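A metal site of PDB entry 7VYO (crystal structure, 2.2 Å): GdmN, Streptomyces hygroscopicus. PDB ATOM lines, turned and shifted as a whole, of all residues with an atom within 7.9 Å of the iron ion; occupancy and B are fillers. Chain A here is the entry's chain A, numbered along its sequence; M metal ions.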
ATOM      1  N   HIS A  27       0.682 -24.580 -22.176  1.00  0.00           N
ATOM      2  CA  HIS A  27       1.163 -25.946 -22.315  1.00  0.00           C
ATOM      3  C   HIS A  27       1.433 -26.571 -20.952  1.00  0.00           C
ATOM      4  O   HIS A  27       1.315 -25.932 -19.906  1.00  0.00           O
ATOM      5  CB  HIS A  27       2.442 -25.910 -23.146  1.00  0.00           C
ATOM      6  CG  HIS A  27       3.391 -24.869 -22.663  1.00  0.00           C
ATOM      7  ND1 HIS A  27       4.227 -25.073 -21.574  1.00  0.00           N
ATOM      8  CD2 HIS A  27       3.573 -23.585 -23.042  1.00  0.00           C
ATOM      9  CE1 HIS A  27       4.910 -23.968 -21.344  1.00  0.00           C
ATOM     10  NE2 HIS A  27       4.532 -23.046 -22.221  1.00  0.00           N
ATOM     11  N   TYR A  82      -4.129 -20.805 -13.121  1.00  0.00           N
ATOM     12  CA  TYR A  82      -2.769 -20.222 -13.006  1.00  0.00           C
ATOM     13  C   TYR A  82      -2.537 -18.898 -13.799  1.00  0.00           C
ATOM     14  O   TYR A  82      -1.351 -18.523 -13.900  1.00  0.00           O
ATOM     15  CB  TYR A  82      -1.737 -21.264 -13.415  1.00  0.00           C
ATOM     16  CG  TYR A  82      -1.607 -21.484 -14.921  1.00  0.00           C
ATOM     17  CD1 TYR A  82      -0.364 -21.761 -15.491  1.00  0.00           C
ATOM     18  CD2 TYR A  82      -2.719 -21.436 -15.771  1.00  0.00           C
ATOM     19  CE1 TYR A  82      -0.230 -21.986 -16.875  1.00  0.00           C
ATOM     20  CE2 TYR A  82      -2.595 -21.642 -17.148  1.00  0.00           C
ATOM     21  CZ  TYR A  82      -1.336 -21.929 -17.682  1.00  0.00           C
ATOM     22  OH  TYR A  82      -1.186 -22.164 -19.030  1.00  0.00           O
ATOM     23  N   PHE A  83      -3.522 -18.197 -14.357  1.00  0.00           N
ATOM     24  CA  PHE A  83      -3.328 -16.918 -15.020  1.00  0.00           C
ATOM     25  C   PHE A  83      -4.507 -16.034 -14.660  1.00  0.00           C
ATOM     26  O   PHE A  83      -5.582 -16.539 -14.305  1.00  0.00           O
ATOM     27  CB  PHE A  83      -3.263 -17.078 -16.550  1.00  0.00           C
ATOM     28  CG  PHE A  83      -1.873 -17.129 -17.126  1.00  0.00           C
ATOM     29  CD1 PHE A  83      -1.223 -15.979 -17.529  1.00  0.00           C
ATOM     30  CD2 PHE A  83      -1.233 -18.342 -17.285  1.00  0.00           C
ATOM     31  CE1 PHE A  83       0.048 -16.033 -18.071  1.00  0.00           C
ATOM     32  CE2 PHE A  83       0.057 -18.405 -17.833  1.00  0.00           C
ATOM     33  CZ  PHE A  83       0.693 -17.241 -18.223  1.00  0.00           C
ATOM     34  N   HIS A 133       0.212 -15.224 -12.496  1.00  0.00           N
ATOM     35  CA  HIS A 133       0.981 -16.407 -12.857  1.00  0.00           C
ATOM     36  C   HIS A 133       2.216 -16.585 -11.972  1.00  0.00           C
ATOM     37  O   HIS A 133       2.496 -17.694 -11.490  1.00  0.00           O
ATOM     38  CB  HIS A 133       1.393 -16.352 -14.321  1.00  0.00           C
ATOM     39  CG  HIS A 133       2.034 -17.612 -14.836  1.00  0.00           C
ATOM     40  ND1 HIS A 133       1.384 -18.825 -14.831  1.00  0.00           N
ATOM     41  CD2 HIS A 133       3.261 -17.846 -15.357  1.00  0.00           C
ATOM     42  CE1 HIS A 133       2.183 -19.750 -15.335  1.00  0.00           C
ATOM     43  NE2 HIS A 133       3.315 -19.174 -15.662  1.00  0.00           N
ATOM     44  N   HIS A 134       2.975 -15.505 -11.758  1.00  0.00           N
ATOM     45  CA  HIS A 134       4.191 -15.665 -10.966  1.00  0.00           C
ATOM     46  C   HIS A 134       3.884 -15.811  -9.481  1.00  0.00           C
ATOM     47  O   HIS A 134       4.673 -16.400  -8.745  1.00  0.00           O
ATOM     48  CB  HIS A 134       5.147 -14.489 -11.210  1.00  0.00           C
ATOM     49  CG  HIS A 134       5.826 -14.559 -12.543  1.00  0.00           C
ATOM     50  ND1 HIS A 134       6.811 -13.684 -12.933  1.00  0.00           N
ATOM     51  CD2 HIS A 134       5.668 -15.423 -13.586  1.00  0.00           C
ATOM     52  CE1 HIS A 134       7.219 -13.982 -14.156  1.00  0.00           C
ATOM     53  NE2 HIS A 134       6.542 -15.035 -14.569  1.00  0.00           N
ATOM     54  N   HIS A 137       3.431 -19.606  -9.271  1.00  0.00           N
ATOM     55  CA  HIS A 137       4.785 -20.188  -9.236  1.00  0.00           C
ATOM     56  C   HIS A 137       5.408 -20.040  -7.859  1.00  0.00           C
ATOM     57  O   HIS A 137       5.937 -21.015  -7.291  1.00  0.00           O
ATOM     58  CB  HIS A 137       5.688 -19.511 -10.274  1.00  0.00           C
ATOM     59  CG  HIS A 137       5.674 -20.168 -11.615  1.00  0.00           C
ATOM     60  ND1 HIS A 137       6.131 -21.463 -11.811  1.00  0.00           N
ATOM     61  CD2 HIS A 137       5.280 -19.724 -12.828  1.00  0.00           C
ATOM     62  CE1 HIS A 137       6.023 -21.776 -13.088  1.00  0.00           C
ATOM     63  NE2 HIS A 137       5.513 -20.731 -13.723  1.00  0.00           N
ATOM     64  N   VAL A 154      11.171 -16.122  -9.342  1.00  0.00           N
ATOM     65  CA  VAL A 154      10.439 -16.777 -10.425  1.00  0.00           C
ATOM     66  C   VAL A 154      10.974 -16.234 -11.728  1.00  0.00           C
ATOM     67  O   VAL A 154      10.899 -15.024 -11.973  1.00  0.00           O
ATOM     68  CB  VAL A 154       8.916 -16.561 -10.339  1.00  0.00           C
ATOM     69  CG1 VAL A 154       8.235 -17.282 -11.504  1.00  0.00           C
ATOM     70  CG2 VAL A 154       8.339 -17.017  -8.973  1.00  0.00           C
ATOM     71  N   LEU A 155      11.478 -17.115 -12.587  1.00  0.00           N
ATOM     72  CA  LEU A 155      11.863 -16.776 -13.962  1.00  0.00           C
ATOM     73  C   LEU A 155      11.298 -17.832 -14.891  1.00  0.00           C
ATOM     74  O   LEU A 155      11.604 -19.017 -14.735  1.00  0.00           O
ATOM     75  CB  LEU A 155      13.386 -16.690 -14.121  1.00  0.00           C
ATOM     76  CG  LEU A 155      14.168 -15.707 -13.275  1.00  0.00           C
ATOM     77  CD1 LEU A 155      15.656 -15.962 -13.436  1.00  0.00           C
ATOM     78  CD2 LEU A 155      13.813 -14.292 -13.708  1.00  0.00           C
ATOM     79  N   ASP A 156      10.497 -17.421 -15.867  1.00  0.00           N
ATOM     80  CA  ASP A 156       9.912 -18.385 -16.803  1.00  0.00           C
ATOM     81  C   ASP A 156       9.890 -17.758 -18.196  1.00  0.00           C
ATOM     82  O   ASP A 156      10.585 -16.767 -18.471  1.00  0.00           O
ATOM     83  CB  ASP A 156       8.531 -18.844 -16.307  1.00  0.00           C
ATOM     84  CG  ASP A 156       7.521 -17.700 -16.227  1.00  0.00           C
ATOM     85  OD1 ASP A 156       6.371 -17.985 -15.874  1.00  0.00           O
ATOM     86  OD2 ASP A 156       7.856 -16.514 -16.490  1.00  0.00           O
ATOM     87  N   GLY A 157       9.101 -18.333 -19.084  1.00  0.00           N
ATOM     88  CA  GLY A 157       8.856 -17.721 -20.374  1.00  0.00           C
ATOM     89  C   GLY A 157       8.141 -16.396 -20.162  1.00  0.00           C
ATOM     90  O   GLY A 157       8.700 -15.344 -20.474  1.00  0.00           O
ATOM     91  N   ARG A 158       6.922 -16.417 -19.603  1.00  0.00           N
ATOM     92  CA  ARG A 158       6.227 -15.189 -19.235  1.00  0.00           C
ATOM     93  C   ARG A 158       5.024 -15.483 -18.339  1.00  0.00           C
ATOM     94  O   ARG A 158       4.420 -16.559 -18.449  1.00  0.00           O
ATOM     95  CB  ARG A 158       5.761 -14.413 -20.482  1.00  0.00           C
ATOM     96  CG  ARG A 158       4.703 -15.146 -21.308  1.00  0.00           C
ATOM     97  CD  ARG A 158       4.103 -14.195 -22.321  1.00  0.00           C
ATOM     98  NE  ARG A 158       3.409 -13.077 -21.671  1.00  0.00           N
ATOM     99  CZ  ARG A 158       2.839 -12.062 -22.305  1.00  0.00           C
ATOM    100  NH1 ARG A 158       2.140 -11.143 -21.660  1.00  0.00           N
ATOM    101  NH2 ARG A 158       2.987 -11.963 -23.625  1.00  0.00           N
ATOM    102  N   GLY A 159       4.700 -14.523 -17.466  1.00  0.00           N
ATOM    103  CA  GLY A 159       3.388 -14.423 -16.862  1.00  0.00           C
ATOM    104  C   GLY A 159       2.514 -13.474 -17.669  1.00  0.00           C
ATOM    105  O   GLY A 159       2.773 -13.218 -18.850  1.00  0.00           O
ATOM    106  N   HIS A 162       4.978 -10.113 -16.819  1.00  0.00           N
ATOM    107  CA  HIS A 162       6.390 -10.135 -16.485  1.00  0.00           C
ATOM    108  C   HIS A 162       7.005 -11.470 -16.896  1.00  0.00           C
ATOM    109  O   HIS A 162       6.329 -12.501 -16.912  1.00  0.00           O
ATOM    110  CB  HIS A 162       6.600  -9.879 -14.981  1.00  0.00           C
ATOM    111  CG  HIS A 162       5.880  -8.668 -14.480  1.00  0.00           C
ATOM    112  ND1 HIS A 162       4.740  -8.741 -13.711  1.00  0.00           N
ATOM    113  CD2 HIS A 162       6.128  -7.339 -14.663  1.00  0.00           C
ATOM    114  CE1 HIS A 162       4.317  -7.519 -13.435  1.00  0.00           C
ATOM    115  NE2 HIS A 162       5.142  -6.655 -14.001  1.00  0.00           N
ATOM    116  N   SER A 163       8.292 -11.428 -17.244  1.00  0.00           N
ATOM    117  CA  SER A 163       9.061 -12.658 -17.429  1.00  0.00           C
ATOM    118  C   SER A 163       9.788 -13.083 -16.162  1.00  0.00           C
ATOM    119  O   SER A 163      10.295 -14.219 -16.117  1.00  0.00           O
ATOM    120  CB  SER A 163      10.071 -12.467 -18.568  1.00  0.00           C
ATOM    121  OG  SER A 163      11.144 -11.629 -18.151  1.00  0.00           O
ATOM    122  N   GLY A 303      11.830 -20.863  -8.668  1.00  0.00           N
ATOM    123  CA  GLY A 303      10.795 -21.489  -9.455  1.00  0.00           C
ATOM    124  C   GLY A 303      10.573 -20.815 -10.785  1.00  0.00           C
ATOM    125  O   GLY A 303      11.310 -19.900 -11.157  1.00  0.00           O
ATOM    126  N   GLY A 304       9.542 -21.239 -11.517  1.00  0.00           N
ATOM    127  CA  GLY A 304       9.431 -20.866 -12.909  1.00  0.00           C
ATOM    128  C   GLY A 304      10.213 -21.828 -13.790  1.00  0.00           C
ATOM    129  O   GLY A 304      11.139 -22.509 -13.342  1.00  0.00           O
ATOM    130  N   GLY A 305       9.843 -21.880 -15.075  1.00  0.00           N
ATOM    131  CA  GLY A 305      10.446 -22.849 -15.977  1.00  0.00           C
ATOM    132  C   GLY A 305      11.960 -22.794 -16.030  1.00  0.00           C
ATOM    133  O   GLY A 305      12.624 -23.830 -16.170  1.00  0.00           O
ATOM    134  N   VAL A 306      12.535 -21.603 -15.871  1.00  0.00           N
ATOM    135  CA  VAL A 306      13.998 -21.486 -15.920  1.00  0.00           C
ATOM    136  C   VAL A 306      14.666 -22.254 -14.784  1.00  0.00           C
ATOM    137  O   VAL A 306      15.813 -22.669 -14.917  1.00  0.00           O
ATOM    138  CB  VAL A 306      14.382 -19.988 -15.932  1.00  0.00           C
ATOM    139  CG1 VAL A 306      15.886 -19.787 -15.927  1.00  0.00           C
ATOM    140  CG2 VAL A 306      13.783 -19.312 -17.170  1.00  0.00           C
ATOM    141  N   SER A 331       8.693 -27.098 -11.498  1.00  0.00           N
ATOM    142  CA  SER A 331       8.857 -25.643 -11.471  1.00  0.00           C
ATOM    143  C   SER A 331       8.285 -24.983 -12.715  1.00  0.00           C
ATOM    144  O   SER A 331       8.162 -23.754 -12.757  1.00  0.00           O
ATOM    145  CB  SER A 331      10.335 -25.278 -11.316  1.00  0.00           C
ATOM    146  OG  SER A 331      10.800 -25.579 -10.009  1.00  0.00           O
ATOM    147  N   HIS A 332       7.912 -25.761 -13.724  1.00  0.00           N
ATOM    148  CA  HIS A 332       7.279 -25.227 -14.918  1.00  0.00           C
ATOM    149  C   HIS A 332       5.798 -25.014 -14.615  1.00  0.00           C
ATOM    150  O   HIS A 332       5.398 -25.002 -13.440  1.00  0.00           O
ATOM    151  CB  HIS A 332       7.509 -26.182 -16.096  1.00  0.00           C
ATOM    152  CG  HIS A 332       6.915 -27.553 -15.892  1.00  0.00           C
ATOM    153  ND1 HIS A 332       6.763 -28.119 -14.645  1.00  0.00           N
ATOM    154  CD2 HIS A 332       6.453 -28.465 -16.775  1.00  0.00           C
ATOM    155  CE1 HIS A 332       6.213 -29.311 -14.767  1.00  0.00           C
ATOM    156  NE2 HIS A 332       6.012 -29.548 -16.050  1.00  0.00           N
ATOM    157  N   ASP A 333       4.961 -24.905 -15.656  1.00  0.00           N
ATOM    158  CA  ASP A 333       3.597 -24.429 -15.432  1.00  0.00           C
ATOM    159  C   ASP A 333       2.723 -25.430 -14.710  1.00  0.00           C
ATOM    160  O   ASP A 333       1.659 -25.038 -14.187  1.00  0.00           O
ATOM    161  CB  ASP A 333       2.958 -24.019 -16.742  1.00  0.00           C
ATOM    162  CG  ASP A 333       3.406 -22.636 -17.184  1.00  0.00           C
ATOM    163  OD1 ASP A 333       3.141 -22.230 -18.332  1.00  0.00           O
ATOM    164  OD2 ASP A 333       4.027 -21.975 -16.344  1.00  0.00           O
ATOM    165  N   ALA A 334       3.106 -26.714 -14.670  1.00  0.00           N
ATOM    166  CA  ALA A 334       2.344 -27.628 -13.831  1.00  0.00           C
ATOM    167  C   ALA A 334       2.438 -27.207 -12.376  1.00  0.00           C
ATOM    168  O   ALA A 334       1.464 -27.316 -11.630  1.00  0.00           O
ATOM    169  CB  ALA A 334       2.824 -29.068 -14.042  1.00  0.00           C
ATOM    170  N   GLY A 335       3.593 -26.667 -11.965  1.00  0.00           N
ATOM    171  CA  GLY A 335       3.750 -26.190 -10.596  1.00  0.00           C
ATOM    172  C   GLY A 335       2.997 -24.900 -10.351  1.00  0.00           C
ATOM    173  O   GLY A 335       2.452 -24.700  -9.261  1.00  0.00           O
ATOM    174  N   ALA A 336       2.926 -24.036 -11.361  1.00  0.00           N
ATOM    175  CA  ALA A 336       2.050 -22.872 -11.242  1.00  0.00           C
ATOM    176  C   ALA A 336       0.597 -23.294 -11.085  1.00  0.00           C
ATOM    177  O   ALA A 336      -0.185 -22.594 -10.436  1.00  0.00           O
ATOM    178  CB  ALA A 336       2.227 -21.959 -12.459  1.00  0.00           C
HETATM  179 FE    FE M   1       5.410 -20.118 -15.989  1.00  0.00          FE
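A ring nitrogen (ND1) of His 133 lies within hydrogen-bond range of the backbone carbonyl oxygen of Tyr 82 (2.9 Å). N of Arg 158 is in hydrogen-bond range of OD2 of Asp 156, at 3.3 Å. OD2 of Asp 156 is in hydrogen-bond range of NE2 of His 134, at 2.8 Å. N of Asp 156 lies within hydrogen-bond range of O of Ser 163, 3.2 Å away. ND1 of His 137 lies close to O of Ser 331 (3.2 Å). ND1 of His 137 sits at hydrogen-bond distance from N of Gly 304, 3.4 Å away.
Within 4 Å of the iron ion: His 133, His 137, Asp 156 and Asp 333. The nearest printed residue that does not touch the iron ion is Arg 158 (4.4 Å).
The iron ion is bound by NE2 of His 133 (2.3 Å), OD1 of Asp 156 (2.3 Å), OD2 of Asp 333 (2.3 Å) and NE2 of His 137 (2.3 Å).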
